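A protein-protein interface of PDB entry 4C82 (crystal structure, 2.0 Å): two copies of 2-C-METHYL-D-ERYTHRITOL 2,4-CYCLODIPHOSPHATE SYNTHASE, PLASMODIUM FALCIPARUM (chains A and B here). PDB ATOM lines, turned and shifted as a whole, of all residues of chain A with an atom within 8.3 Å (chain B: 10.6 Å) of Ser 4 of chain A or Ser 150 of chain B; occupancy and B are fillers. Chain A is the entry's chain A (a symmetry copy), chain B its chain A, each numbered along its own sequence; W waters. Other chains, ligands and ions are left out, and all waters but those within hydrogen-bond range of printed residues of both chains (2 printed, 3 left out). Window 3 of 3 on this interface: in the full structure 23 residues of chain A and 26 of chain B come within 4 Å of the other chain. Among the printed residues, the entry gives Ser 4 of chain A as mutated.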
ATOM      1  N   SER A   4     -17.899 -20.243 -11.088  1.00  0.00           N
ATOM      2  CA  SER A   4     -19.225 -20.436 -10.419  1.00  0.00           C
ATOM      3  C   SER A   4     -19.146 -20.157  -8.889  1.00  0.00           C
ATOM      4  O   SER A   4     -18.372 -20.801  -8.162  1.00  0.00           O
ATOM      5  CB  SER A   4     -19.762 -21.843 -10.711  1.00  0.00           C
ATOM      6  OG  SER A   4     -20.954 -22.122  -9.979  1.00  0.00           O
ATOM      7  N   TYR A   5     -19.957 -19.212  -8.404  1.00  0.00           N
ATOM      8  CA  TYR A   5     -19.831 -18.786  -7.028  1.00  0.00           C
ATOM      9  C   TYR A   5     -20.685 -19.690  -6.184  1.00  0.00           C
ATOM     10  O   TYR A   5     -21.869 -19.938  -6.487  1.00  0.00           O
ATOM     11  CB  TYR A   5     -20.165 -17.284  -6.877  1.00  0.00           C
ATOM     12  CG  TYR A   5     -20.249 -16.759  -5.444  1.00  0.00           C
ATOM     13  CD1 TYR A   5     -19.107 -16.517  -4.705  1.00  0.00           C
ATOM     14  CD2 TYR A   5     -21.511 -16.546  -4.824  1.00  0.00           C
ATOM     15  CE1 TYR A   5     -19.190 -16.085  -3.371  1.00  0.00           C
ATOM     16  CE2 TYR A   5     -21.608 -16.107  -3.515  1.00  0.00           C
ATOM     17  CZ  TYR A   5     -20.471 -15.834  -2.785  1.00  0.00           C
ATOM     18  OH  TYR A   5     -20.538 -15.380  -1.466  1.00  0.00           O
ATOM     19  N   ASN A   6     -20.079 -20.227  -5.129  1.00  0.00           N
ATOM     20  CA  ASN A   6     -20.817 -21.076  -4.184  1.00  0.00           C
ATOM     21  C   ASN A   6     -20.660 -20.590  -2.777  1.00  0.00           C
ATOM     22  O   ASN A   6     -20.902 -21.342  -1.840  1.00  0.00           O
ATOM     23  CB  ASN A   6     -20.369 -22.563  -4.274  1.00  0.00           C
ATOM     24  CG  ASN A   6     -20.797 -23.212  -5.569  1.00  0.00           C
ATOM     25  OD1 ASN A   6     -21.914 -23.755  -5.686  1.00  0.00           O
ATOM     26  ND2 ASN A   6     -19.923 -23.159  -6.563  1.00  0.00           N
ATOM     27  N   GLY A   7     -20.294 -19.328  -2.569  1.00  0.00           N
ATOM     28  CA  GLY A   7     -20.290 -18.831  -1.163  1.00  0.00           C
ATOM     29  C   GLY A   7     -21.733 -18.444  -0.729  1.00  0.00           C
ATOM     30  O   GLY A   7     -22.709 -18.676  -1.474  1.00  0.00           O
ATOM     31  N   ARG A   9     -25.136 -16.425  -0.147  1.00  0.00           N
ATOM     32  CA  ARG A   9     -25.858 -15.600  -1.130  1.00  0.00           C
ATOM     33  C   ARG A   9     -26.987 -14.817  -0.491  1.00  0.00           C
ATOM     34  O   ARG A   9     -27.669 -15.343   0.404  1.00  0.00           O
ATOM     35  CB  ARG A   9     -26.385 -16.428  -2.309  1.00  0.00           C
ATOM     36  CG  ARG A   9     -25.299 -16.848  -3.343  1.00  0.00           C
ATOM     37  CD  ARG A   9     -25.855 -17.965  -4.236  1.00  0.00           C
ATOM     38  NE  ARG A   9     -25.025 -18.269  -5.410  1.00  0.00           N
ATOM     39  CZ  ARG A   9     -24.882 -17.570  -6.524  1.00  0.00           C
ATOM     40  NH1 ARG A   9     -25.539 -16.410  -6.740  1.00  0.00           N
ATOM     41  NH2 ARG A   9     -24.044 -18.061  -7.483  1.00  0.00           N
ATOM     42  N   GLY A  75     -33.670 -14.812  -6.938  1.00  0.00           N
ATOM     43  CA  GLY A  75     -32.717 -13.765  -7.024  1.00  0.00           C
ATOM     44  C   GLY A  75     -31.404 -14.155  -6.356  1.00  0.00           C
ATOM     45  O   GLY A  75     -30.314 -13.873  -6.879  1.00  0.00           O
ATOM     46  N   ALA A  76     -31.483 -14.745  -5.166  1.00  0.00           N
ATOM     47  CA  ALA A  76     -30.259 -15.141  -4.546  1.00  0.00           C
ATOM     48  C   ALA A  76     -29.407 -16.008  -5.474  1.00  0.00           C
ATOM     49  O   ALA A  76     -28.189 -15.881  -5.518  1.00  0.00           O
ATOM     50  CB  ALA A  76     -30.536 -15.826  -3.215  1.00  0.00           C
ATOM     51  N   LEU A  77     -30.063 -16.864  -6.260  1.00  0.00           N
ATOM     52  CA  LEU A  77     -29.321 -17.873  -7.034  1.00  0.00           C
ATOM     53  C   LEU A  77     -29.079 -17.471  -8.463  1.00  0.00           C
ATOM     54  O   LEU A  77     -28.385 -18.177  -9.187  1.00  0.00           O
ATOM     55  CB  LEU A  77     -30.111 -19.131  -7.041  1.00  0.00           C
ATOM     56  CG  LEU A  77     -30.180 -19.705  -5.667  1.00  0.00           C
ATOM     57  CD1 LEU A  77     -31.370 -20.676  -5.691  1.00  0.00           C
ATOM     58  CD2 LEU A  77     -28.845 -20.376  -5.346  1.00  0.00           C
ATOM     59  N   GLY A  78     -29.646 -16.338  -8.876  1.00  0.00           N
ATOM     60  CA  GLY A  78     -29.457 -15.852 -10.231  1.00  0.00           C
ATOM     61  C   GLY A  78     -30.313 -16.533 -11.302  1.00  0.00           C
ATOM     62  O   GLY A  78     -29.953 -16.462 -12.490  1.00  0.00           O
ATOM     63  N   SER A  79     -31.447 -17.154 -10.936  1.00  0.00           N
ATOM     64  CA  SER A  79     -32.365 -17.671 -11.960  1.00  0.00           C
ATOM     65  C   SER A  79     -33.215 -16.600 -12.680  1.00  0.00           C
ATOM     66  O   SER A  79     -33.398 -15.509 -12.166  1.00  0.00           O
ATOM     67  CB  SER A  79     -33.326 -18.681 -11.337  1.00  0.00           C
ATOM     68  OG  SER A  79     -32.537 -19.602 -10.630  1.00  0.00           O
ATOM     69  N   LYS A 112     -28.894 -26.996  -5.947  1.00  0.00           N
ATOM     70  CA  LYS A 112     -27.695 -26.124  -6.010  1.00  0.00           C
ATOM     71  C   LYS A 112     -26.765 -26.303  -4.825  1.00  0.00           C
ATOM     72  O   LYS A 112     -25.774 -25.569  -4.703  1.00  0.00           O
ATOM     73  CB  LYS A 112     -28.093 -24.621  -6.072  1.00  0.00           C
ATOM     74  CG  LYS A 112     -28.999 -24.262  -7.247  1.00  0.00           C
ATOM     75  CD  LYS A 112     -28.310 -24.567  -8.555  1.00  0.00           C
ATOM     76  CE  LYS A 112     -27.377 -23.452  -8.989  1.00  0.00           C
ATOM     77  NZ  LYS A 112     -28.035 -22.571 -10.002  1.00  0.00           N
ATOM     78  N   TYR A 114     -27.500 -25.663  -1.430  1.00  0.00           N
ATOM     79  CA  TYR A 114     -27.625 -24.612  -0.409  1.00  0.00           C
ATOM     80  C   TYR A 114     -28.635 -25.013   0.622  1.00  0.00           C
ATOM     81  O   TYR A 114     -29.476 -25.880   0.352  1.00  0.00           O
ATOM     82  CB  TYR A 114     -28.085 -23.342  -1.108  1.00  0.00           C
ATOM     83  CG  TYR A 114     -26.936 -22.580  -1.677  1.00  0.00           C
ATOM     84  CD1 TYR A 114     -26.271 -21.638  -0.897  1.00  0.00           C
ATOM     85  CD2 TYR A 114     -26.559 -22.735  -3.017  1.00  0.00           C
ATOM     86  CE1 TYR A 114     -25.186 -20.951  -1.420  1.00  0.00           C
ATOM     87  CE2 TYR A 114     -25.522 -21.999  -3.560  1.00  0.00           C
ATOM     88  CZ  TYR A 114     -24.824 -21.127  -2.739  1.00  0.00           C
ATOM     89  OH  TYR A 114     -23.778 -20.372  -3.234  1.00  0.00           O
ATOM     90  N   ILE B 116     -16.818  -9.388  -4.146  1.00  0.00           N
ATOM     91  CA  ILE B 116     -18.264  -9.420  -4.146  1.00  0.00           C
ATOM     92  C   ILE B 116     -18.699 -10.884  -4.037  1.00  0.00           C
ATOM     93  O   ILE B 116     -18.075 -11.743  -4.711  1.00  0.00           O
ATOM     94  CB  ILE B 116     -18.788  -8.863  -5.488  1.00  0.00           C
ATOM     95  CG1 ILE B 116     -18.534  -7.344  -5.474  1.00  0.00           C
ATOM     96  CG2 ILE B 116     -20.268  -9.256  -5.614  1.00  0.00           C
ATOM     97  CD1 ILE B 116     -18.751  -6.600  -6.791  1.00  0.00           C
ATOM     98  N   GLY B 117     -19.681 -11.191  -3.169  1.00  0.00           N
ATOM     99  CA  GLY B 117     -20.389 -12.499  -3.188  1.00  0.00           C
ATOM    100  C   GLY B 117     -21.352 -12.544  -4.345  1.00  0.00           C
ATOM    101  O   GLY B 117     -21.027 -13.030  -5.424  1.00  0.00           O
ATOM    102  N   ASN B 118     -22.585 -12.044  -4.132  1.00  0.00           N
ATOM    103  CA  ASN B 118     -23.490 -11.949  -5.260  1.00  0.00           C
ATOM    104  C   ASN B 118     -24.240 -10.617  -5.140  1.00  0.00           C
ATOM    105  O   ASN B 118     -24.155  -9.940  -4.112  1.00  0.00           O
ATOM    106  CB  ASN B 118     -24.455 -13.135  -5.314  1.00  0.00           C
ATOM    107  CG  ASN B 118     -25.538 -13.066  -4.188  1.00  0.00           C
ATOM    108  OD1 ASN B 118     -25.204 -13.050  -3.003  1.00  0.00           O
ATOM    109  ND2 ASN B 118     -26.813 -12.929  -4.583  1.00  0.00           N
ATOM    110  N   VAL B 119     -24.930 -10.217  -6.201  1.00  0.00           N
ATOM    111  CA  VAL B 119     -25.708  -8.968  -6.111  1.00  0.00           C
ATOM    112  C   VAL B 119     -27.126  -9.354  -6.649  1.00  0.00           C
ATOM    113  O   VAL B 119     -27.212 -10.135  -7.558  1.00  0.00           O
ATOM    114  CB  VAL B 119     -25.041  -7.848  -6.916  1.00  0.00           C
ATOM    115  CG1 VAL B 119     -24.861  -8.280  -8.368  1.00  0.00           C
ATOM    116  CG2 VAL B 119     -25.872  -6.506  -6.824  1.00  0.00           C
ATOM    117  N   ASP B 120     -28.202  -8.897  -6.002  1.00  0.00           N
ATOM    118  CA  ASP B 120     -29.564  -9.150  -6.463  1.00  0.00           C
ATOM    119  C   ASP B 120     -30.207  -7.727  -6.607  1.00  0.00           C
ATOM    120  O   ASP B 120     -30.181  -6.963  -5.676  1.00  0.00           O
ATOM    121  CB  ASP B 120     -30.275 -10.035  -5.492  1.00  0.00           C
ATOM    122  CG  ASP B 120     -31.671 -10.480  -6.003  1.00  0.00           C
ATOM    123  OD1 ASP B 120     -31.944 -10.404  -7.233  1.00  0.00           O
ATOM    124  OD2 ASP B 120     -32.463 -10.899  -5.155  1.00  0.00           O
ATOM    125  N   LYS B 135     -30.310 -10.298 -20.133  1.00  0.00           N
ATOM    126  CA  LYS B 135     -28.937 -10.817 -20.502  1.00  0.00           C
ATOM    127  C   LYS B 135     -27.874  -9.725 -20.763  1.00  0.00           C
ATOM    128  O   LYS B 135     -26.722  -9.813 -20.310  1.00  0.00           O
ATOM    129  CB  LYS B 135     -28.980 -11.823 -21.666  1.00  0.00           C
ATOM    130  CG  LYS B 135     -28.675 -13.249 -21.253  1.00  0.00           C
ATOM    131  CD  LYS B 135     -27.177 -13.503 -21.172  1.00  0.00           C
ATOM    132  CE  LYS B 135     -26.878 -14.958 -20.848  1.00  0.00           C
ATOM    133  NZ  LYS B 135     -25.414 -15.225 -20.807  1.00  0.00           N
ATOM    134  N   ILE B 138     -26.813  -8.020 -17.492  1.00  0.00           N
ATOM    135  CA  ILE B 138     -26.035  -8.870 -16.602  1.00  0.00           C
ATOM    136  C   ILE B 138     -24.590  -8.945 -17.119  1.00  0.00           C
ATOM    137  O   ILE B 138     -23.621  -8.853 -16.325  1.00  0.00           O
ATOM    138  CB  ILE B 138     -26.679 -10.250 -16.459  1.00  0.00           C
ATOM    139  CG1 ILE B 138     -27.958 -10.157 -15.594  1.00  0.00           C
ATOM    140  CG2 ILE B 138     -25.697 -11.260 -15.842  1.00  0.00           C
ATOM    141  CD1 ILE B 138     -28.821 -11.447 -15.573  1.00  0.00           C
ATOM    142  N   LYS B 139     -24.437  -9.036 -18.441  1.00  0.00           N
ATOM    143  CA  LYS B 139     -23.094  -9.081 -19.031  1.00  0.00           C
ATOM    144  C   LYS B 139     -22.406  -7.767 -18.780  1.00  0.00           C
ATOM    145  O   LYS B 139     -21.204  -7.756 -18.513  1.00  0.00           O
ATOM    146  CB  LYS B 139     -23.170  -9.367 -20.557  1.00  0.00           C
ATOM    147  CG  LYS B 139     -21.800  -9.710 -21.115  1.00  0.00           C
ATOM    148  CD  LYS B 139     -21.440  -8.828 -22.293  1.00  0.00           C
ATOM    149  CE  LYS B 139     -19.919  -8.785 -22.500  1.00  0.00           C
ATOM    150  NZ  LYS B 139     -19.571  -7.860 -23.617  1.00  0.00           N
ATOM    151  N   ILE B 141     -22.957  -5.562 -16.278  1.00  0.00           N
ATOM    152  CA  ILE B 141     -22.543  -5.517 -14.869  1.00  0.00           C
ATOM    153  C   ILE B 141     -21.309  -6.392 -14.603  1.00  0.00           C
ATOM    154  O   ILE B 141     -20.367  -5.984 -13.892  1.00  0.00           O
ATOM    155  CB  ILE B 141     -23.701  -5.969 -13.938  1.00  0.00           C
ATOM    156  CG1 ILE B 141     -24.819  -4.930 -14.007  1.00  0.00           C
ATOM    157  CG2 ILE B 141     -23.190  -6.145 -12.486  1.00  0.00           C
ATOM    158  CD1 ILE B 141     -26.109  -5.443 -13.389  1.00  0.00           C
ATOM    159  N   SER B 142     -21.335  -7.608 -15.144  1.00  0.00           N
ATOM    160  CA  SER B 142     -20.277  -8.513 -14.867  1.00  0.00           C
ATOM    161  C   SER B 142     -18.931  -7.986 -15.417  1.00  0.00           C
ATOM    162  O   SER B 142     -17.943  -8.036 -14.703  1.00  0.00           O
ATOM    163  CB  SER B 142     -20.628  -9.932 -15.269  1.00  0.00           C
ATOM    164  OG  SER B 142     -20.236 -10.227 -16.558  1.00  0.00           O
ATOM    165  N   THR B 143     -18.948  -7.315 -16.577  1.00  0.00           N
ATOM    166  CA  THR B 143     -17.748  -6.659 -17.118  1.00  0.00           C
ATOM    167  C   THR B 143     -17.272  -5.479 -16.287  1.00  0.00           C
ATOM    168  O   THR B 143     -16.079  -5.367 -15.974  1.00  0.00           O
ATOM    169  CB  THR B 143     -18.013  -6.132 -18.540  1.00  0.00           C
ATOM    170  OG1 THR B 143     -18.501  -7.205 -19.347  1.00  0.00           O
ATOM    171  CG2 THR B 143     -16.725  -5.479 -19.159  1.00  0.00           C
ATOM    172  N   ASN B 146     -16.231  -6.941 -12.881  1.00  0.00           N
ATOM    173  CA  ASN B 146     -15.263  -7.975 -13.091  1.00  0.00           C
ATOM    174  C   ASN B 146     -15.598  -9.162 -12.250  1.00  0.00           C
ATOM    175  O   ASN B 146     -14.786  -9.591 -11.419  1.00  0.00           O
ATOM    176  CB  ASN B 146     -13.832  -7.464 -12.803  1.00  0.00           C
ATOM    177  CG  ASN B 146     -12.783  -8.487 -13.169  1.00  0.00           C
ATOM    178  OD1 ASN B 146     -12.802  -9.023 -14.278  1.00  0.00           O
ATOM    179  ND2 ASN B 146     -11.909  -8.818 -12.229  1.00  0.00           N
ATOM    180  N   ILE B 147     -16.820  -9.687 -12.422  1.00  0.00           N
ATOM    181  CA  ILE B 147     -17.225 -10.842 -11.614  1.00  0.00           C
ATOM    182  C   ILE B 147     -17.970 -11.708 -12.590  1.00  0.00           C
ATOM    183  O   ILE B 147     -18.328 -11.236 -13.653  1.00  0.00           O
ATOM    184  CB  ILE B 147     -18.138 -10.442 -10.400  1.00  0.00           C
ATOM    185  CG1 ILE B 147     -19.441  -9.738 -10.842  1.00  0.00           C
ATOM    186  CG2 ILE B 147     -17.364  -9.581  -9.397  1.00  0.00           C
ATOM    187  CD1 ILE B 147     -20.456  -9.333  -9.778  1.00  0.00           C
ATOM    188  N   ASP B 148     -18.268 -12.935 -12.213  1.00  0.00           N
ATOM    189  CA  ASP B 148     -18.973 -13.839 -13.071  1.00  0.00           C
ATOM    190  C   ASP B 148     -20.490 -13.536 -13.188  1.00  0.00           C
ATOM    191  O   ASP B 148     -21.125 -12.949 -12.277  1.00  0.00           O
ATOM    192  CB  ASP B 148     -18.762 -15.267 -12.551  1.00  0.00           C
ATOM    193  CG  ASP B 148     -19.133 -16.300 -13.575  1.00  0.00           C
ATOM    194  OD1 ASP B 148     -18.386 -16.374 -14.571  1.00  0.00           O
ATOM    195  OD2 ASP B 148     -20.176 -17.012 -13.434  1.00  0.00           O
ATOM    196  N   GLU B 149     -21.078 -13.964 -14.299  1.00  0.00           N
ATOM    197  CA  GLU B 149     -22.505 -13.765 -14.529  1.00  0.00           C
ATOM    198  C   GLU B 149     -23.338 -14.546 -13.501  1.00  0.00           C
ATOM    199  O   GLU B 149     -24.420 -14.112 -13.134  1.00  0.00           O
ATOM    200  CB  GLU B 149     -22.913 -14.035 -16.005  1.00  0.00           C
ATOM    201  CG  GLU B 149     -22.206 -13.085 -17.001  1.00  0.00           C
ATOM    202  CD  GLU B 149     -22.798 -13.070 -18.426  1.00  0.00           C
ATOM    203  OE1 GLU B 149     -23.858 -13.681 -18.668  1.00  0.00           O
ATOM    204  OE2 GLU B 149     -22.210 -12.431 -19.319  1.00  0.00           O
ATOM    205  N   SER B 150     -22.819 -15.668 -12.993  1.00  0.00           N
ATOM    206  CA  SER B 150     -23.504 -16.389 -11.939  1.00  0.00           C
ATOM    207  C   SER B 150     -23.600 -15.647 -10.566  1.00  0.00           C
ATOM    208  O   SER B 150     -24.210 -16.145  -9.643  1.00  0.00           O
ATOM    209  CB  SER B 150     -22.856 -17.752 -11.745  1.00  0.00           C
ATOM    210  OG  SER B 150     -21.515 -17.593 -11.346  1.00  0.00           O
ATOM    211  N   GLN B 151     -22.919 -14.518 -10.414  1.00  0.00           N
ATOM    212  CA  GLN B 151     -22.982 -13.764  -9.146  1.00  0.00           C
ATOM    213  C   GLN B 151     -24.030 -12.618  -9.259  1.00  0.00           C
ATOM    214  O   GLN B 151     -24.207 -11.891  -8.315  1.00  0.00           O
ATOM    215  CB  GLN B 151     -21.608 -13.211  -8.775  1.00  0.00           C
ATOM    216  CG  GLN B 151     -20.576 -14.369  -8.396  1.00  0.00           C
ATOM    217  CD  GLN B 151     -19.154 -13.797  -8.379  1.00  0.00           C
ATOM    218  OE1 GLN B 151     -18.464 -13.793  -9.406  1.00  0.00           O
ATOM    219  NE2 GLN B 151     -18.809 -13.126  -7.288  1.00  0.00           N
ATOM    220  N   ILE B 152     -24.710 -12.526 -10.411  1.00  0.00           N
ATOM    221  CA  ILE B 152     -25.624 -11.399 -10.695  1.00  0.00           C
ATOM    222  C   ILE B 152     -27.056 -11.886 -10.954  1.00  0.00           C
ATOM    223  O   ILE B 152     -27.310 -12.912 -11.637  1.00  0.00           O
ATOM    224  CB  ILE B 152     -25.112 -10.552 -11.876  1.00  0.00           C
ATOM    225  CG1 ILE B 152     -23.636 -10.189 -11.658  1.00  0.00           C
ATOM    226  CG2 ILE B 152     -26.028  -9.345 -12.160  1.00  0.00           C
ATOM    227  CD1 ILE B 152     -22.914  -9.895 -12.956  1.00  0.00           C
ATOM    228  N   SER B 153     -28.021 -11.134 -10.424  1.00  0.00           N
ATOM    229  CA  SER B 153     -29.439 -11.437 -10.711  1.00  0.00           C
ATOM    230  C   SER B 153     -30.041 -10.066 -11.007  1.00  0.00           C
ATOM    231  O   SER B 153     -29.730  -9.122 -10.260  1.00  0.00           O
ATOM    232  CB  SER B 153     -30.104 -11.962  -9.482  1.00  0.00           C
ATOM    233  OG  SER B 153     -31.536 -11.807  -9.616  1.00  0.00           O
ATOM    234  N   VAL B 154     -30.805  -9.921 -12.091  1.00  0.00           N
ATOM    235  CA  VAL B 154     -31.458  -8.640 -12.325  1.00  0.00           C
ATOM    236  C   VAL B 154     -32.929  -9.005 -12.608  1.00  0.00           C
ATOM    237  O   VAL B 154     -33.170  -9.811 -13.512  1.00  0.00           O
ATOM    238  CB  VAL B 154     -30.875  -7.821 -13.511  1.00  0.00           C
ATOM    239  CG1 VAL B 154     -29.431  -7.435 -13.343  1.00  0.00           C
ATOM    240  CG2 VAL B 154     -31.012  -8.554 -14.809  1.00  0.00           C
HETATM  241  O   HOH W   1     -26.093 -18.401 -10.323  1.00  0.00           O
HETATM  242  O   HOH W   2     -26.657 -15.157  -8.616  1.00  0.00           O
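Among the printed residues, merely in contact across the chains: Ser 4 of chain A with Ser 150 of chain B, Tyr 5 of chain A with Gly 117 of chain B, Tyr 5 of chain A with Ser 150 of chain B, Tyr 5 of chain A with Gln 151 of chain B, Arg 9 of chain A with Asn 118 of chain B, Gly 75 of chain A with Asp 120 of chain B, Gly 75 of chain A with Ser 153 of chain B, Ala 76 of chain A with Asp 120 of chain B and Gly 78 of chain A with Ile 152 of chain B.
The backbone carbonyl oxygen (O) of Tyr 5 of chain A sits at hydrogen-bond distance from the guanidinium group (NH2) of Arg 9 of chain A (3.0 Å).
The side-chain amide nitrogen (NE2) of Gln 151 of chain B lies within hydrogen-bond range of the backbone carbonyl oxygen (O) of Ile 116 of chain B.
The backbone carbonyl oxygen (O) of Val 119 of chain B sits at hydrogen-bond distance from the backbone NH (N) of Ser 153 of chain B.
The side-chain hydroxyl of Ser 153 of chain B sits at hydrogen-bond distance from the side-chain carboxylate of Asp 120 of chain B.
The backbone carbonyl oxygen of Gln 151 of chain B is in hydrogen-bond range of the backbone NH of Val 119 of chain B.
OH of Tyr 114 of chain A is in hydrogen-bond range of NE of Arg 9 of chain A, 3.3 Å away.
The guanidinium group (NH2) of Arg 9 of chain A sits at hydrogen-bond distance from the backbone carbonyl oxygen (O) of Ser 150 of chain B (2.9 Å).
The side-chain amide nitrogen (ND2) of Asn 118 of chain B sits at hydrogen-bond distance from the backbone carbonyl oxygen (O) of Ala 76 of chain A, at 3.4 Å.
No position is printed for both chains.
Ser 4 of chain A touches just one residue of chain B: Ser 150.
Printed residues of chain B within 4 Å of Tyr 5 of chain A: Gly 117 (3.4 Å), Ser 150 (3.7 Å) and Gln 151 (3.3 Å).
Of the printed residues of chain A, Asn 118 of chain B touches Arg 9 (3.2 Å) and Ala 76 (3.4 Å).
Of the printed residues of chain A, Asp 120 of chain B touches Gly 75 and Ala 76.
Ser 150 of chain B touches three residues of chain A.
Of the printed residues of chain A, Ser 153 of chain B touches Gly 75.
Water W2 lies within hydrogen-bond range of the guanidinium group of Arg 9 of chain A, the backbone carbonyl oxygen of Ser 150 of chain B and the backbone NH of Gly 78 of chain A.
Water W1 bridges the backbone carbonyl oxygen (O) of Leu 77 of chain A and the backbone carbonyl oxygen (O) of Ser 150 of chain B.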
